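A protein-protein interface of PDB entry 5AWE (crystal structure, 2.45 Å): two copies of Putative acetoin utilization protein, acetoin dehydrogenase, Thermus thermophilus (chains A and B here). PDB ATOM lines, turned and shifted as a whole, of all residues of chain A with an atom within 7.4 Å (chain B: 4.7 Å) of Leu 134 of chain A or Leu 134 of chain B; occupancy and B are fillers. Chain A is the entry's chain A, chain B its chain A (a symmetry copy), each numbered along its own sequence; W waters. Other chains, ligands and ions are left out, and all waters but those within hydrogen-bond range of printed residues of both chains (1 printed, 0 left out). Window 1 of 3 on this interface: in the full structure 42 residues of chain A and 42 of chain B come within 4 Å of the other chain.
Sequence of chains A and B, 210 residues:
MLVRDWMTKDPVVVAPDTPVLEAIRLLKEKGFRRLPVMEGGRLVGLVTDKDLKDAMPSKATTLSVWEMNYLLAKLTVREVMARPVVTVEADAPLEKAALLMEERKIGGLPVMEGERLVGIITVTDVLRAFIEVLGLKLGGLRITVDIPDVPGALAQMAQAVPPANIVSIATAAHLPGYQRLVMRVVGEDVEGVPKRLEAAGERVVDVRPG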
ATOM      1  N   MET A   1      17.909 -20.715  20.919  1.00  0.00           N
ATOM      2  CA  MET A   1      18.587 -21.043  22.201  1.00  0.00           C
ATOM      3  C   MET A   1      19.983 -21.561  21.889  1.00  0.00           C
ATOM      4  O   MET A   1      20.175 -22.749  21.634  1.00  0.00           O
ATOM      5  CB  MET A   1      17.814 -22.123  22.962  1.00  0.00           C
ATOM      6  CG  MET A   1      16.338 -21.847  23.128  1.00  0.00           C
ATOM      7  SD  MET A   1      15.499 -23.275  23.808  1.00  0.00           S
ATOM      8  CE  MET A   1      16.489 -23.549  25.285  1.00  0.00           C
ATOM      9  N   GLU A  95      20.801 -26.291  25.376  1.00  0.00           N
ATOM     10  CA  GLU A  95      20.566 -27.558  26.088  1.00  0.00           C
ATOM     11  C   GLU A  95      21.794 -28.476  26.141  1.00  0.00           C
ATOM     12  O   GLU A  95      21.906 -29.326  27.031  1.00  0.00           O
ATOM     13  CB  GLU A  95      19.396 -28.338  25.455  1.00  0.00           C
ATOM     14  CG  GLU A  95      18.089 -27.564  25.335  1.00  0.00           C
ATOM     15  CD  GLU A  95      17.905 -26.932  23.961  1.00  0.00           C
ATOM     16  OE1 GLU A  95      17.095 -27.454  23.176  1.00  0.00           O
ATOM     17  OE2 GLU A  95      18.566 -25.913  23.660  1.00  0.00           O
ATOM     18  N   ARG A 128      19.113 -19.170  33.917  1.00  0.00           N
ATOM     19  CA  ARG A 128      18.483 -17.986  33.346  1.00  0.00           C
ATOM     20  C   ARG A 128      17.779 -18.343  32.024  1.00  0.00           C
ATOM     21  O   ARG A 128      16.629 -17.962  31.795  1.00  0.00           O
ATOM     22  CB  ARG A 128      19.544 -16.900  33.113  1.00  0.00           C
ATOM     23  CG  ARG A 128      18.967 -15.493  32.970  1.00  0.00           C
ATOM     24  CD  ARG A 128      20.027 -14.404  33.169  1.00  0.00           C
ATOM     25  NE  ARG A 128      20.982 -14.349  32.064  1.00  0.00           N
ATOM     26  CZ  ARG A 128      22.197 -14.889  32.106  1.00  0.00           C
ATOM     27  NH1 ARG A 128      22.599 -15.520  33.207  1.00  0.00           N
ATOM     28  NH2 ARG A 128      23.007 -14.808  31.053  1.00  0.00           N
ATOM     29  N   ALA A 129      18.470 -19.093  31.172  1.00  0.00           N
ATOM     30  CA  ALA A 129      17.947 -19.448  29.858  1.00  0.00           C
ATOM     31  C   ALA A 129      16.636 -20.226  29.963  1.00  0.00           C
ATOM     32  O   ALA A 129      15.659 -19.906  29.283  1.00  0.00           O
ATOM     33  CB  ALA A 129      18.986 -20.272  29.088  1.00  0.00           C
ATOM     34  N   PHE A 130      16.616 -21.247  30.819  1.00  0.00           N
ATOM     35  CA  PHE A 130      15.421 -22.065  30.990  1.00  0.00           C
ATOM     36  C   PHE A 130      14.311 -21.228  31.592  1.00  0.00           C
ATOM     37  O   PHE A 130      13.143 -21.402  31.264  1.00  0.00           O
ATOM     38  CB  PHE A 130      15.712 -23.272  31.888  1.00  0.00           C
ATOM     39  CG  PHE A 130      16.442 -24.391  31.189  1.00  0.00           C
ATOM     40  CD1 PHE A 130      16.046 -24.819  29.928  1.00  0.00           C
ATOM     41  CD2 PHE A 130      17.524 -25.019  31.796  1.00  0.00           C
ATOM     42  CE1 PHE A 130      16.719 -25.859  29.272  1.00  0.00           C
ATOM     43  CE2 PHE A 130      18.202 -26.058  31.154  1.00  0.00           C
ATOM     44  CZ  PHE A 130      17.797 -26.479  29.887  1.00  0.00           C
ATOM     45  N   ILE A 131      14.688 -20.303  32.460  1.00  0.00           N
ATOM     46  CA  ILE A 131      13.725 -19.416  33.086  1.00  0.00           C
ATOM     47  C   ILE A 131      13.086 -18.517  32.031  1.00  0.00           C
ATOM     48  O   ILE A 131      11.892 -18.220  32.093  1.00  0.00           O
ATOM     49  CB  ILE A 131      14.405 -18.554  34.160  1.00  0.00           C
ATOM     50  CG1 ILE A 131      14.818 -19.435  35.337  1.00  0.00           C
ATOM     51  CG2 ILE A 131      13.478 -17.443  34.611  1.00  0.00           C
ATOM     52  CD1 ILE A 131      15.737 -18.740  36.342  1.00  0.00           C
ATOM     53  N   GLU A 132      13.877 -18.101  31.052  1.00  0.00           N
ATOM     54  CA  GLU A 132      13.358 -17.247  29.999  1.00  0.00           C
ATOM     55  C   GLU A 132      12.485 -18.022  29.000  1.00  0.00           C
ATOM     56  O   GLU A 132      11.339 -17.643  28.740  1.00  0.00           O
ATOM     57  CB  GLU A 132      14.514 -16.575  29.260  1.00  0.00           C
ATOM     58  CG  GLU A 132      14.080 -15.663  28.126  1.00  0.00           C
ATOM     59  CD  GLU A 132      15.209 -14.766  27.648  1.00  0.00           C
ATOM     60  OE1 GLU A 132      15.323 -14.557  26.421  1.00  0.00           O
ATOM     61  OE2 GLU A 132      15.983 -14.273  28.501  1.00  0.00           O
ATOM     62  N   VAL A 133      13.017 -19.108  28.443  1.00  0.00           N
ATOM     63  CA  VAL A 133      12.342 -19.768  27.339  1.00  0.00           C
ATOM     64  C   VAL A 133      11.098 -20.538  27.778  1.00  0.00           C
ATOM     65  O   VAL A 133      10.208 -20.789  26.966  1.00  0.00           O
ATOM     66  CB  VAL A 133      13.295 -20.716  26.559  1.00  0.00           C
ATOM     67  CG1 VAL A 133      14.566 -19.967  26.183  1.00  0.00           C
ATOM     68  CG2 VAL A 133      13.591 -21.972  27.356  1.00  0.00           C
ATOM     69  N   LEU A 134      11.023 -20.892  29.057  1.00  0.00           N
ATOM     70  CA  LEU A 134       9.838 -21.568  29.585  1.00  0.00           C
ATOM     71  C   LEU A 134       8.858 -20.564  30.213  1.00  0.00           C
ATOM     72  O   LEU A 134       7.740 -20.922  30.580  1.00  0.00           O
ATOM     73  CB  LEU A 134      10.245 -22.622  30.627  1.00  0.00           C
ATOM     74  CG  LEU A 134      11.296 -23.690  30.262  1.00  0.00           C
ATOM     75  CD1 LEU A 134      11.519 -24.603  31.463  1.00  0.00           C
ATOM     76  CD2 LEU A 134      10.853 -24.515  29.071  1.00  0.00           C
ATOM     77  N   GLY A 135       9.290 -19.310  30.337  1.00  0.00           N
ATOM     78  CA  GLY A 135       8.395 -18.257  30.789  1.00  0.00           C
ATOM     79  C   GLY A 135       8.078 -18.285  32.279  1.00  0.00           C
ATOM     80  O   GLY A 135       6.974 -17.925  32.684  1.00  0.00           O
ATOM     81  N   LEU A 136       9.037 -18.704  33.098  1.00  0.00           N
ATOM     82  CA  LEU A 136       8.776 -18.927  34.516  1.00  0.00           C
ATOM     83  C   LEU A 136       8.560 -17.601  35.238  1.00  0.00           C
ATOM     84  O   LEU A 136       8.166 -17.569  36.405  1.00  0.00           O
ATOM     85  CB  LEU A 136       9.945 -19.693  35.160  1.00  0.00           C
ATOM     86  CG  LEU A 136      10.397 -20.991  34.470  1.00  0.00           C
ATOM     87  CD1 LEU A 136      11.494 -21.654  35.288  1.00  0.00           C
ATOM     88  CD2 LEU A 136       9.218 -21.939  34.292  1.00  0.00           C
ATOM     89  N   LYS A 137       8.818 -16.505  34.539  1.00  0.00           N
ATOM     90  CA  LYS A 137       8.653 -15.181  35.116  1.00  0.00           C
ATOM     91  C   LYS A 137       7.508 -14.403  34.479  1.00  0.00           C
ATOM     92  O   LYS A 137       7.352 -13.214  34.741  1.00  0.00           O
ATOM     93  CB  LYS A 137       9.945 -14.376  34.963  1.00  0.00           C
ATOM     94  CG  LYS A 137      10.991 -14.648  36.020  1.00  0.00           C
ATOM     95  CD  LYS A 137      12.241 -13.831  35.747  1.00  0.00           C
ATOM     96  CE  LYS A 137      13.179 -13.841  36.948  1.00  0.00           C
ATOM     97  NZ  LYS A 137      12.565 -13.201  38.151  1.00  0.00           N
ATOM     98  N   LEU A 138       6.715 -15.064  33.639  1.00  0.00           N
ATOM     99  CA  LEU A 138       5.666 -14.373  32.890  1.00  0.00           C
ATOM    100  C   LEU A 138       4.304 -14.384  33.566  1.00  0.00           C
ATOM    101  O   LEU A 138       3.318 -13.925  32.982  1.00  0.00           O
ATOM    102  CB  LEU A 138       5.527 -14.969  31.490  1.00  0.00           C
ATOM    103  CG  LEU A 138       6.751 -14.834  30.585  1.00  0.00           C
ATOM    104  CD1 LEU A 138       6.382 -15.328  29.201  1.00  0.00           C
ATOM    105  CD2 LEU A 138       7.220 -13.373  30.539  1.00  0.00           C
ATOM    106  N   VAL A 167       2.953 -20.676  26.260  1.00  0.00           N
ATOM    107  CA  VAL A 167       4.352 -20.249  26.177  1.00  0.00           C
ATOM    108  C   VAL A 167       5.324 -21.429  26.267  1.00  0.00           C
ATOM    109  O   VAL A 167       6.410 -21.399  25.676  1.00  0.00           O
ATOM    110  CB  VAL A 167       4.672 -19.220  27.285  1.00  0.00           C
ATOM    111  CG1 VAL A 167       6.152 -18.888  27.296  1.00  0.00           C
ATOM    112  CG2 VAL A 167       3.865 -17.952  27.038  1.00  0.00           C
ATOM    113  N   SER A 168       4.931 -22.469  27.003  1.00  0.00           N
ATOM    114  CA  SER A 168       5.753 -23.670  27.093  1.00  0.00           C
ATOM    115  C   SER A 168       5.006 -24.873  27.636  1.00  0.00           C
ATOM    116  O   SER A 168       4.103 -24.750  28.465  1.00  0.00           O
ATOM    117  CB  SER A 168       6.990 -23.415  27.965  1.00  0.00           C
ATOM    118  OG  SER A 168       6.618 -23.227  29.317  1.00  0.00           O
ATOM    119  N   ILE A 169       5.407 -26.042  27.152  1.00  0.00           N
ATOM    120  CA  ILE A 169       4.860 -27.311  27.604  1.00  0.00           C
ATOM    121  C   ILE A 169       6.014 -28.223  27.985  1.00  0.00           C
ATOM    122  O   ILE A 169       6.987 -28.352  27.228  1.00  0.00           O
ATOM    123  CB  ILE A 169       4.021 -27.983  26.491  1.00  0.00           C
ATOM    124  CG1 ILE A 169       2.755 -27.161  26.239  1.00  0.00           C
ATOM    125  CG2 ILE A 169       3.648 -29.401  26.888  1.00  0.00           C
ATOM    126  CD1 ILE A 169       2.003 -27.562  24.985  1.00  0.00           C
ATOM    127  N   ALA A 170       5.910 -28.834  29.165  1.00  0.00           N
ATOM    128  CA  ALA A 170       6.839 -29.884  29.572  1.00  0.00           C
ATOM    129  C   ALA A 170       6.099 -31.162  29.965  1.00  0.00           C
ATOM    130  O   ALA A 170       4.941 -31.115  30.429  1.00  0.00           O
ATOM    131  CB  ALA A 170       7.699 -29.406  30.725  1.00  0.00           C
ATOM    132  N   THR A 171       6.770 -32.302  29.778  1.00  0.00           N
ATOM    133  CA  THR A 171       6.214 -33.597  30.177  1.00  0.00           C
ATOM    134  C   THR A 171       6.656 -33.957  31.592  1.00  0.00           C
ATOM    135  O   THR A 171       7.797 -34.351  31.807  1.00  0.00           O
ATOM    136  CB  THR A 171       6.672 -34.727  29.221  1.00  0.00           C
ATOM    137  OG1 THR A 171       6.253 -34.419  27.891  1.00  0.00           O
ATOM    138  CG2 THR A 171       6.063 -36.067  29.631  1.00  0.00           C
ATOM    139  N   ALA A 172       5.756 -33.825  32.559  1.00  0.00           N
ATOM    140  CA  ALA A 172       6.099 -34.178  33.934  1.00  0.00           C
ATOM    141  C   ALA A 172       6.274 -35.685  34.066  1.00  0.00           C
ATOM    142  O   ALA A 172       7.084 -36.150  34.869  1.00  0.00           O
ATOM    143  CB  ALA A 172       5.022 -33.693  34.894  1.00  0.00           C
ATOM    144  N   MET A 183       2.076 -26.982  31.789  1.00  0.00           N
ATOM    145  CA  MET A 183       1.833 -26.048  30.699  1.00  0.00           C
ATOM    146  C   MET A 183       1.718 -24.658  31.295  1.00  0.00           C
ATOM    147  O   MET A 183       1.038 -24.463  32.296  1.00  0.00           O
ATOM    148  CB  MET A 183       0.531 -26.422  29.965  1.00  0.00           C
ATOM    149  CG  MET A 183       0.268 -25.650  28.669  1.00  0.00           C
ATOM    150  SD  MET A 183      -1.419 -25.899  28.013  1.00  0.00           S
ATOM    151  CE  MET A 183      -1.097 -25.952  26.381  1.00  0.00           C
ATOM    152  N   ARG A 184       2.401 -23.692  30.695  1.00  0.00           N
ATOM    153  CA  ARG A 184       2.263 -22.315  31.130  1.00  0.00           C
ATOM    154  C   ARG A 184       1.536 -21.523  30.073  1.00  0.00           C
ATOM    155  O   ARG A 184       1.928 -21.516  28.911  1.00  0.00           O
ATOM    156  CB  ARG A 184       3.638 -21.708  31.429  1.00  0.00           C
ATOM    157  CG  ARG A 184       4.167 -22.154  32.777  1.00  0.00           C
ATOM    158  CD  ARG A 184       5.608 -21.781  33.008  1.00  0.00           C
ATOM    159  NE  ARG A 184       6.085 -22.372  34.261  1.00  0.00           N
ATOM    160  CZ  ARG A 184       5.893 -21.838  35.467  1.00  0.00           C
ATOM    161  NH1 ARG A 184       5.232 -20.694  35.597  1.00  0.00           N
ATOM    162  NH2 ARG A 184       6.365 -22.445  36.547  1.00  0.00           N
ATOM    163  N   VAL A 185       0.451 -20.881  30.482  1.00  0.00           N
ATOM    164  CA  VAL A 185      -0.386 -20.132  29.561  1.00  0.00           C
ATOM    165  C   VAL A 185      -0.493 -18.696  30.050  1.00  0.00           C
ATOM    166  O   VAL A 185      -0.448 -18.438  31.257  1.00  0.00           O
ATOM    167  CB  VAL A 185      -1.800 -20.752  29.462  1.00  0.00           C
ATOM    168  CG1 VAL A 185      -1.712 -22.172  28.860  1.00  0.00           C
ATOM    169  CG2 VAL A 185      -2.448 -20.795  30.849  1.00  0.00           C
ATOM    170  N   PHE B 130      15.086 -30.499  34.502  1.00  0.00           N
ATOM    171  CA  PHE B 130      14.781 -29.875  33.221  1.00  0.00           C
ATOM    172  C   PHE B 130      15.180 -30.804  32.092  1.00  0.00           C
ATOM    173  O   PHE B 130      14.516 -30.867  31.064  1.00  0.00           O
ATOM    174  CB  PHE B 130      15.511 -28.536  33.079  1.00  0.00           C
ATOM    175  CG  PHE B 130      14.868 -27.405  33.842  1.00  0.00           C
ATOM    176  CD1 PHE B 130      13.495 -27.206  33.793  1.00  0.00           C
ATOM    177  CD2 PHE B 130      15.640 -26.537  34.607  1.00  0.00           C
ATOM    178  CE1 PHE B 130      12.889 -26.157  34.498  1.00  0.00           C
ATOM    179  CE2 PHE B 130      15.050 -25.487  35.314  1.00  0.00           C
ATOM    180  CZ  PHE B 130      13.668 -25.297  35.258  1.00  0.00           C
ATOM    181  N   ILE B 131      16.259 -31.540  32.303  1.00  0.00           N
ATOM    182  CA  ILE B 131      16.729 -32.491  31.312  1.00  0.00           C
ATOM    183  C   ILE B 131      15.702 -33.605  31.134  1.00  0.00           C
ATOM    184  O   ILE B 131      15.479 -34.086  30.022  1.00  0.00           O
ATOM    185  CB  ILE B 131      18.077 -33.091  31.739  1.00  0.00           C
ATOM    186  CG1 ILE B 131      19.161 -32.016  31.669  1.00  0.00           C
ATOM    187  CG2 ILE B 131      18.430 -34.276  30.863  1.00  0.00           C
ATOM    188  CD1 ILE B 131      20.482 -32.421  32.323  1.00  0.00           C
ATOM    189  N   GLU B 132      15.065 -34.002  32.227  1.00  0.00           N
ATOM    190  CA  GLU B 132      14.066 -35.052  32.155  1.00  0.00           C
ATOM    191  C   GLU B 132      12.749 -34.561  31.534  1.00  0.00           C
ATOM    192  O   GLU B 132      12.247 -35.153  30.573  1.00  0.00           O
ATOM    193  CB  GLU B 132      13.799 -35.609  33.553  1.00  0.00           C
ATOM    194  CG  GLU B 132      12.757 -36.711  33.593  1.00  0.00           C
ATOM    195  CD  GLU B 132      12.766 -37.462  34.915  1.00  0.00           C
ATOM    196  OE1 GLU B 132      11.672 -37.798  35.416  1.00  0.00           O
ATOM    197  OE2 GLU B 132      13.870 -37.712  35.452  1.00  0.00           O
ATOM    198  N   VAL B 133      12.191 -33.477  32.071  1.00  0.00           N
ATOM    199  CA  VAL B 133      10.849 -33.079  31.682  1.00  0.00           C
ATOM    200  C   VAL B 133      10.791 -32.477  30.279  1.00  0.00           C
ATOM    201  O   VAL B 133       9.734 -32.478  29.650  1.00  0.00           O
ATOM    202  CB  VAL B 133      10.220 -32.089  32.702  1.00  0.00           C
ATOM    203  CG1 VAL B 133      10.342 -32.658  34.109  1.00  0.00           C
ATOM    204  CG2 VAL B 133      10.848 -30.713  32.589  1.00  0.00           C
ATOM    205  N   LEU B 134      11.923 -31.986  29.782  1.00  0.00           N
ATOM    206  CA  LEU B 134      11.980 -31.456  28.420  1.00  0.00           C
ATOM    207  C   LEU B 134      12.468 -32.524  27.427  1.00  0.00           C
ATOM    208  O   LEU B 134      12.444 -32.314  26.216  1.00  0.00           O
ATOM    209  CB  LEU B 134      12.905 -30.230  28.364  1.00  0.00           C
ATOM    210  CG  LEU B 134      12.675 -29.056  29.337  1.00  0.00           C
ATOM    211  CD1 LEU B 134      13.723 -27.978  29.077  1.00  0.00           C
ATOM    212  CD2 LEU B 134      11.288 -28.468  29.173  1.00  0.00           C
ATOM    213  N   GLY B 135      12.912 -33.665  27.953  1.00  0.00           N
ATOM    214  CA  GLY B 135      13.265 -34.788  27.099  1.00  0.00           C
ATOM    215  C   GLY B 135      14.582 -34.631  26.349  1.00  0.00           C
ATOM    216  O   GLY B 135      14.717 -35.115  25.228  1.00  0.00           O
ATOM    217  N   LEU B 136      15.555 -33.961  26.960  1.00  0.00           N
ATOM    218  CA  LEU B 136      16.787 -33.613  26.261  1.00  0.00           C
ATOM    219  C   LEU B 136      17.629 -34.858  26.002  1.00  0.00           C
ATOM    220  O   LEU B 136      18.628 -34.811  25.284  1.00  0.00           O
ATOM    221  CB  LEU B 136      17.595 -32.591  27.080  1.00  0.00           C
ATOM    222  CG  LEU B 136      16.853 -31.331  27.556  1.00  0.00           C
ATOM    223  CD1 LEU B 136      17.823 -30.400  28.267  1.00  0.00           C
ATOM    224  CD2 LEU B 136      16.199 -30.620  26.377  1.00  0.00           C
ATOM    225  N   VAL B 167       7.066 -33.875  23.012  1.00  0.00           N
ATOM    226  CA  VAL B 167       7.447 -34.072  24.412  1.00  0.00           C
ATOM    227  C   VAL B 167       7.607 -32.745  25.160  1.00  0.00           C
ATOM    228  O   VAL B 167       7.355 -32.668  26.369  1.00  0.00           O
ATOM    229  CB  VAL B 167       8.754 -34.890  24.509  1.00  0.00           C
ATOM    230  CG1 VAL B 167       9.232 -34.969  25.946  1.00  0.00           C
ATOM    231  CG2 VAL B 167       8.506 -36.295  23.975  1.00  0.00           C
ATOM    232  N   SER B 168       8.023 -31.703  24.441  1.00  0.00           N
ATOM    233  CA  SER B 168       8.138 -30.380  25.045  1.00  0.00           C
ATOM    234  C   SER B 168       8.244 -29.260  24.028  1.00  0.00           C
ATOM    235  O   SER B 168       8.798 -29.428  22.939  1.00  0.00           O
ATOM    236  CB  SER B 168       9.349 -30.318  25.985  1.00  0.00           C
ATOM    237  OG  SER B 168      10.556 -30.398  25.251  1.00  0.00           O
ATOM    238  N   ALA B 170       9.287 -25.047  23.940  1.00  0.00           N
ATOM    239  CA  ALA B 170       9.757 -23.816  24.569  1.00  0.00           C
ATOM    240  C   ALA B 170       9.712 -22.639  23.594  1.00  0.00           C
ATOM    241  O   ALA B 170       9.836 -22.820  22.365  1.00  0.00           O
ATOM    242  CB  ALA B 170      11.167 -24.000  25.096  1.00  0.00           C
ATOM    243  N   ARG B 184      10.610 -30.471  20.791  1.00  0.00           N
ATOM    244  CA  ARG B 184      11.210 -31.789  20.698  1.00  0.00           C
ATOM    245  C   ARG B 184      10.139 -32.814  20.424  1.00  0.00           C
ATOM    246  O   ARG B 184       9.149 -32.898  21.144  1.00  0.00           O
ATOM    247  CB  ARG B 184      11.976 -32.119  21.984  1.00  0.00           C
ATOM    248  CG  ARG B 184      13.325 -31.430  22.026  1.00  0.00           C
ATOM    249  CD  ARG B 184      14.006 -31.529  23.366  1.00  0.00           C
ATOM    250  NE  ARG B 184      15.227 -30.718  23.370  1.00  0.00           N
ATOM    251  CZ  ARG B 184      16.403 -31.124  22.891  1.00  0.00           C
ATOM    252  NH1 ARG B 184      16.531 -32.337  22.367  1.00  0.00           N
ATOM    253  NH2 ARG B 184      17.456 -30.320  22.941  1.00  0.00           N
HETATM  254  O   HOH W   1      14.381 -28.040  24.304  1.00  0.00           O
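The side-chain carboxylate (OE1) of Glu 95 of chain A is in salt-bridge range of the guanidinium group (NH2) of Arg 184 of chain B. The backbone NH (N) of Thr 171 of chain A is in hydrogen-bond range of the backbone carbonyl oxygen (O) of Val 133 of chain B (3.0 Å). The side-chain hydroxyl of Thr 171 of chain A sits at hydrogen-bond distance from the backbone carbonyl oxygen of Val 167 of chain B, at 2.6 Å.
OG of Ser 168 of chain A lies within hydrogen-bond range of O of Leu 134 of chain A. The backbone carbonyl oxygen (O) of Ile 131 of chain B sits at hydrogen-bond distance from the backbone NH (N) of Leu 136 of chain B, 3.1 Å away. The backbone carbonyl oxygen (O) of Leu 134 of chain B lies within hydrogen-bond range of the side-chain hydroxyl (OG) of Ser 168 of chain B, at 2.9 Å. N of Val 167 of chain B lies within hydrogen-bond range of O of Arg 184 of chain B (3.0 Å). O of Ser 168 of chain B lies within hydrogen-bond range of N of Arg 184 of chain B (3.0 Å).
Glu 95 of chain A touches Leu 136 of chain B. Phe 130 of chain A touches Phe 130 of chain B. Phe 130 of chain A touches Leu 134 of chain B. Val 133 of chain A touches Ala 170 of chain B. Phe 130 of chain B touches Leu 134 of chain A. Leu 134 of chain A touches Leu 134 of chain B (CD2 to CD2, 3.98 Å). Ser 168 of chain B touches Ile 169 of chain A (CA to O, 3.2 Å). CB of Ala 170 of chain A touches O of Val 133 of chain B (3.8 Å).
Leu 134 of chain A touches just these residues of chain B: Phe 130 (3.7 Å) and Leu 134 (3.98 Å). Printed residues of chain A within 4 Å of Phe 130 of chain B: Phe 130 (3.7 Å) and Leu 134 (3.7 Å). Of the printed residues of chain B, Thr 171 of chain A touches Val 133 (3.0 Å) and Val 167 (2.6 Å). Of the printed residues of chain B, Phe 130 of chain A touches Phe 130 (3.7 Å) and Leu 134 (3.7 Å). Of the printed residues of chain A, Arg 184 of chain B touches Glu 95. Printed residues of chain A within 4 Å of Val 133 of chain B: Ala 170 (3.8 Å) and Thr 171 (3.0 Å). Met 183 of chain A touches none of the printed residues of chain B. Glu 132 of chain A touches none of the printed residues of chain B. The nearest residue of chain B that does not touch Leu 134 of chain A is Ala 170 of chain B (4.02 Å).
Of the 11 printed residues of chain B, 8 touch a printed residue of chain A. Hydrophobic or aromatic side chains of chain B within 4 Å of the printed part of chain A: Phe 130, Val 133, Leu 134, Leu 136, Val 167 and Ala 170. Hydrophobic or aromatic side chains of chain A that line the printed part of chain B: Phe 130, Val 133, Leu 134 and Ala 170. Among the printed residues, 11 pairs touch across the chains. Among the printed residues, Asp or Glu carboxylates within 4 Å of a Lys or Arg side-chain nitrogen of the other chain: Glu 95 of chain A with Arg 184 of chain B (2.9 Å).
Phe 130 of chain B touches its own counterpart, Phe 130 of chain A. Phe 130 of chain A touches Leu 134 of chain B, and with the chains exchanged Leu 134 of chain A touches Phe 130 of chain B. Val 133 of chain A touches Ala 170 of chain B, and with the chains exchanged Ala 170 of chain A touches Val 133 of chain B. Leu 134 of chain A touches its own counterpart, Leu 134 of chain B. 11 positions are printed for both chains. Of the 11 pairs that touch across the chains among the printed residues, 6 have their exchanged pair printed and touching as well.
Water W1 lies within hydrogen-bond range of NE of Arg 184 of chain B (3.0 Å) and OE1 of Glu 95 of chain A (3.0 Å).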
